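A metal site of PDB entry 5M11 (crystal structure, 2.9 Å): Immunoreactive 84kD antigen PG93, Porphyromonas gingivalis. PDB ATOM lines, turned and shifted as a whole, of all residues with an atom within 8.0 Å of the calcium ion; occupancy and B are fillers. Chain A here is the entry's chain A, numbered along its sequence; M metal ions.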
ATOM      1  N   TRP A 436     -16.364 -33.291   0.454  1.00  0.00           N
ATOM      2  CA  TRP A 436     -17.307 -33.809  -0.517  1.00  0.00           C
ATOM      3  C   TRP A 436     -17.231 -35.339  -0.482  1.00  0.00           C
ATOM      4  O   TRP A 436     -16.152 -35.921  -0.283  1.00  0.00           O
ATOM      5  CB  TRP A 436     -16.992 -33.271  -1.909  1.00  0.00           C
ATOM      6  CG  TRP A 436     -17.240 -31.818  -2.005  1.00  0.00           C
ATOM      7  CD1 TRP A 436     -16.389 -30.810  -1.668  1.00  0.00           C
ATOM      8  CD2 TRP A 436     -18.484 -31.189  -2.358  1.00  0.00           C
ATOM      9  NE1 TRP A 436     -17.008 -29.595  -1.815  1.00  0.00           N
ATOM     10  CE2 TRP A 436     -18.282 -29.791  -2.273  1.00  0.00           C
ATOM     11  CE3 TRP A 436     -19.737 -31.680  -2.771  1.00  0.00           C
ATOM     12  CZ2 TRP A 436     -19.293 -28.887  -2.566  1.00  0.00           C
ATOM     13  CZ3 TRP A 436     -20.733 -30.766  -3.081  1.00  0.00           C
ATOM     14  CH2 TRP A 436     -20.516 -29.390  -2.961  1.00  0.00           C
ATOM     15  N   PHE A 459     -27.441 -33.691  -1.994  1.00  0.00           N
ATOM     16  CA  PHE A 459     -28.212 -33.592  -3.234  1.00  0.00           C
ATOM     17  C   PHE A 459     -27.906 -34.796  -4.133  1.00  0.00           C
ATOM     18  O   PHE A 459     -27.145 -35.681  -3.739  1.00  0.00           O
ATOM     19  CB  PHE A 459     -27.893 -32.258  -3.964  1.00  0.00           C
ATOM     20  CG  PHE A 459     -26.446 -32.046  -4.371  1.00  0.00           C
ATOM     21  CD1 PHE A 459     -25.970 -32.550  -5.576  1.00  0.00           C
ATOM     22  CD2 PHE A 459     -25.589 -31.292  -3.586  1.00  0.00           C
ATOM     23  CE1 PHE A 459     -24.637 -32.353  -5.966  1.00  0.00           C
ATOM     24  CE2 PHE A 459     -24.272 -31.073  -3.989  1.00  0.00           C
ATOM     25  CZ  PHE A 459     -23.803 -31.598  -5.182  1.00  0.00           C
ATOM     26  N   TYR A 461     -28.489 -36.163  -8.773  1.00  0.00           N
ATOM     27  CA  TYR A 461     -28.956 -35.945 -10.129  1.00  0.00           C
ATOM     28  C   TYR A 461     -29.752 -37.204 -10.520  1.00  0.00           C
ATOM     29  O   TYR A 461     -29.197 -38.286 -10.378  1.00  0.00           O
ATOM     30  CB  TYR A 461     -27.787 -35.650 -11.064  1.00  0.00           C
ATOM     31  CG  TYR A 461     -26.887 -34.532 -10.577  1.00  0.00           C
ATOM     32  CD1 TYR A 461     -27.267 -33.201 -10.689  1.00  0.00           C
ATOM     33  CD2 TYR A 461     -25.641 -34.812 -10.000  1.00  0.00           C
ATOM     34  CE1 TYR A 461     -26.442 -32.167 -10.240  1.00  0.00           C
ATOM     35  CE2 TYR A 461     -24.808 -33.788  -9.556  1.00  0.00           C
ATOM     36  CZ  TYR A 461     -25.201 -32.465  -9.696  1.00  0.00           C
ATOM     37  OH  TYR A 461     -24.371 -31.450  -9.284  1.00  0.00           O
ATOM     38  N   ASN A 501     -20.374 -29.901 -11.094  1.00  0.00           N
ATOM     39  CA  ASN A 501     -19.925 -28.688 -10.420  1.00  0.00           C
ATOM     40  C   ASN A 501     -21.088 -28.029  -9.710  1.00  0.00           C
ATOM     41  O   ASN A 501     -22.024 -27.543 -10.343  1.00  0.00           O
ATOM     42  CB  ASN A 501     -19.253 -27.711 -11.389  1.00  0.00           C
ATOM     43  CG  ASN A 501     -18.292 -26.778 -10.702  1.00  0.00           C
ATOM     44  OD1 ASN A 501     -18.678 -25.937  -9.884  1.00  0.00           O
ATOM     45  ND2 ASN A 501     -17.020 -26.891 -11.035  1.00  0.00           N
ATOM     46  N   ASP A 502     -21.026 -28.053  -8.368  1.00  0.00           N
ATOM     47  CA  ASP A 502     -21.999 -27.498  -7.421  1.00  0.00           C
ATOM     48  C   ASP A 502     -22.191 -25.965  -7.568  1.00  0.00           C
ATOM     49  O   ASP A 502     -23.161 -25.428  -7.030  1.00  0.00           O
ATOM     50  CB  ASP A 502     -21.527 -27.820  -5.999  1.00  0.00           C
ATOM     51  CG  ASP A 502     -20.220 -27.128  -5.649  1.00  0.00           C
ATOM     52  OD1 ASP A 502     -19.199 -27.378  -6.363  1.00  0.00           O
ATOM     53  OD2 ASP A 502     -20.211 -26.327  -4.680  1.00  0.00           O
ATOM     54  N   ARG A 503     -21.226 -25.281  -8.229  1.00  0.00           N
ATOM     55  CA  ARG A 503     -21.157 -23.836  -8.521  1.00  0.00           C
ATOM     56  C   ARG A 503     -21.236 -22.988  -7.213  1.00  0.00           C
ATOM     57  O   ARG A 503     -21.976 -21.997  -7.148  1.00  0.00           O
ATOM     58  CB  ARG A 503     -22.249 -23.400  -9.549  1.00  0.00           C
ATOM     59  CG  ARG A 503     -22.165 -24.064 -10.932  1.00  0.00           C
ATOM     60  CD  ARG A 503     -20.885 -23.715 -11.671  1.00  0.00           C
ATOM     61  NE  ARG A 503     -20.914 -24.100 -13.082  1.00  0.00           N
ATOM     62  CZ  ARG A 503     -19.865 -24.543 -13.768  1.00  0.00           C
ATOM     63  NH1 ARG A 503     -18.683 -24.680 -13.174  1.00  0.00           N
ATOM     64  NH2 ARG A 503     -19.985 -24.860 -15.045  1.00  0.00           N
ATOM     65  N   GLY A 504     -20.469 -23.394  -6.203  1.00  0.00           N
ATOM     66  CA  GLY A 504     -20.387 -22.715  -4.915  1.00  0.00           C
ATOM     67  C   GLY A 504     -21.565 -22.840  -3.962  1.00  0.00           C
ATOM     68  O   GLY A 504     -21.449 -22.447  -2.799  1.00  0.00           O
ATOM     69  N   THR A 505     -22.701 -23.364  -4.431  1.00  0.00           N
ATOM     70  CA  THR A 505     -23.906 -23.511  -3.610  1.00  0.00           C
ATOM     71  C   THR A 505     -24.294 -25.012  -3.466  1.00  0.00           C
ATOM     72  O   THR A 505     -25.020 -25.549  -4.315  1.00  0.00           O
ATOM     73  CB  THR A 505     -25.047 -22.684  -4.213  1.00  0.00           C
ATOM     74  OG1 THR A 505     -25.202 -23.044  -5.587  1.00  0.00           O
ATOM     75  CG2 THR A 505     -24.828 -21.189  -4.074  1.00  0.00           C
ATOM     76  N   PRO A 506     -23.829 -25.716  -2.400  1.00  0.00           N
ATOM     77  CA  PRO A 506     -24.219 -27.137  -2.238  1.00  0.00           C
ATOM     78  C   PRO A 506     -25.688 -27.310  -1.785  1.00  0.00           C
ATOM     79  O   PRO A 506     -26.192 -28.436  -1.780  1.00  0.00           O
ATOM     80  CB  PRO A 506     -23.236 -27.648  -1.179  1.00  0.00           C
ATOM     81  CG  PRO A 506     -22.874 -26.457  -0.381  1.00  0.00           C
ATOM     82  CD  PRO A 506     -22.950 -25.261  -1.297  1.00  0.00           C
ATOM     83  N   GLU A 507     -26.365 -26.207  -1.443  1.00  0.00           N
ATOM     84  CA  GLU A 507     -27.763 -26.192  -1.018  1.00  0.00           C
ATOM     85  C   GLU A 507     -28.767 -26.163  -2.237  1.00  0.00           C
ATOM     86  O   GLU A 507     -29.968 -26.377  -2.038  1.00  0.00           O
ATOM     87  CB  GLU A 507     -28.039 -25.026  -0.026  1.00  0.00           C
ATOM     88  CG  GLU A 507     -27.982 -23.624  -0.612  1.00  0.00           C
ATOM     89  CD  GLU A 507     -26.629 -22.974  -0.867  1.00  0.00           C
ATOM     90  OE1 GLU A 507     -25.580 -23.608  -0.581  1.00  0.00           O
ATOM     91  OE2 GLU A 507     -26.631 -21.815  -1.346  1.00  0.00           O
ATOM     92  N   THR A 508     -28.260 -25.905  -3.473  1.00  0.00           N
ATOM     93  CA  THR A 508     -29.083 -25.935  -4.701  1.00  0.00           C
ATOM     94  C   THR A 508     -28.387 -26.686  -5.836  1.00  0.00           C
ATOM     95  O   THR A 508     -27.161 -26.770  -5.905  1.00  0.00           O
ATOM     96  CB  THR A 508     -29.519 -24.540  -5.211  1.00  0.00           C
ATOM     97  OG1 THR A 508     -29.074 -23.487  -4.340  1.00  0.00           O
ATOM     98  CG2 THR A 508     -31.024 -24.454  -5.446  1.00  0.00           C
ATOM     99  N   THR A 509     -29.232 -27.223  -6.731  1.00  0.00           N
ATOM    100  CA  THR A 509     -28.909 -27.970  -7.942  1.00  0.00           C
ATOM    101  C   THR A 509     -29.267 -27.065  -9.127  1.00  0.00           C
ATOM    102  O   THR A 509     -28.719 -27.238 -10.218  1.00  0.00           O
ATOM    103  CB  THR A 509     -29.734 -29.270  -7.906  1.00  0.00           C
ATOM    104  OG1 THR A 509     -29.284 -30.035  -6.794  1.00  0.00           O
ATOM    105  CG2 THR A 509     -29.633 -30.100  -9.189  1.00  0.00           C
ATOM    106  N   SER A 510     -30.167 -26.085  -8.882  1.00  0.00           N
ATOM    107  CA  SER A 510     -30.739 -25.149  -9.861  1.00  0.00           C
ATOM    108  C   SER A 510     -29.664 -24.374 -10.673  1.00  0.00           C
ATOM    109  O   SER A 510     -29.952 -23.997 -11.811  1.00  0.00           O
ATOM    110  CB  SER A 510     -31.694 -24.170  -9.174  1.00  0.00           C
ATOM    111  OG  SER A 510     -31.073 -23.087  -8.499  1.00  0.00           O
ATOM    112  N   ASP A 511     -28.457 -24.160 -10.096  1.00  0.00           N
ATOM    113  CA  ASP A 511     -27.352 -23.435 -10.740  1.00  0.00           C
ATOM    114  C   ASP A 511     -26.181 -24.360 -11.167  1.00  0.00           C
ATOM    115  O   ASP A 511     -25.264 -23.894 -11.846  1.00  0.00           O
ATOM    116  CB  ASP A 511     -26.832 -22.299  -9.829  1.00  0.00           C
ATOM    117  CG  ASP A 511     -26.195 -22.695  -8.498  1.00  0.00           C
ATOM    118  OD1 ASP A 511     -26.807 -23.493  -7.750  1.00  0.00           O
ATOM    119  OD2 ASP A 511     -25.132 -22.130  -8.169  1.00  0.00           O
ATOM    120  N   ASP A 512     -26.240 -25.651 -10.791  1.00  0.00           N
ATOM    121  CA  ASP A 512     -25.231 -26.663 -11.109  1.00  0.00           C
ATOM    122  C   ASP A 512     -25.100 -26.973 -12.585  1.00  0.00           C
ATOM    123  O   ASP A 512     -26.033 -26.780 -13.362  1.00  0.00           O
ATOM    124  CB  ASP A 512     -25.548 -27.976 -10.401  1.00  0.00           C
ATOM    125  CG  ASP A 512     -25.301 -27.948  -8.918  1.00  0.00           C
ATOM    126  OD1 ASP A 512     -25.284 -26.836  -8.346  1.00  0.00           O
ATOM    127  OD2 ASP A 512     -25.156 -29.030  -8.320  1.00  0.00           O
ATOM    128  N   SER A 513     -23.908 -27.481 -12.945  1.00  0.00           N
ATOM    129  CA  SER A 513     -23.484 -28.018 -14.239  1.00  0.00           C
ATOM    130  C   SER A 513     -23.026 -29.451 -13.994  1.00  0.00           C
ATOM    131  O   SER A 513     -22.255 -29.693 -13.061  1.00  0.00           O
ATOM    132  CB  SER A 513     -22.343 -27.187 -14.835  1.00  0.00           C
ATOM    133  OG  SER A 513     -22.714 -25.855 -15.171  1.00  0.00           O
HETATM  134 CA    CA M   1     -25.508 -25.178  -6.637  1.00  0.00          CA
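The side-chain carboxylate (OD2) of Asp 512 sits at hydrogen-bond distance from the side-chain hydroxyl (OH) of Tyr 461 (2.7 Å).
The backbone NH (N) of Gly 504 is in hydrogen-bond range of the side-chain carboxylate (OD2) of Asp 502, at 3.3 Å.
The calcium ion is bound by OD1 of Asp 512, O of Asp 502, OG1 of Thr 505, O of Thr 505, OD1 of Asp 511 and O of Thr 508.
The calcium ion has six donor atoms within binding distance.
Along chain A the residues within 4 Å of the calcium ion span positions 502 to 512.
The nearest printed residue that does not touch the calcium ion is Thr 509 (4.2 Å).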
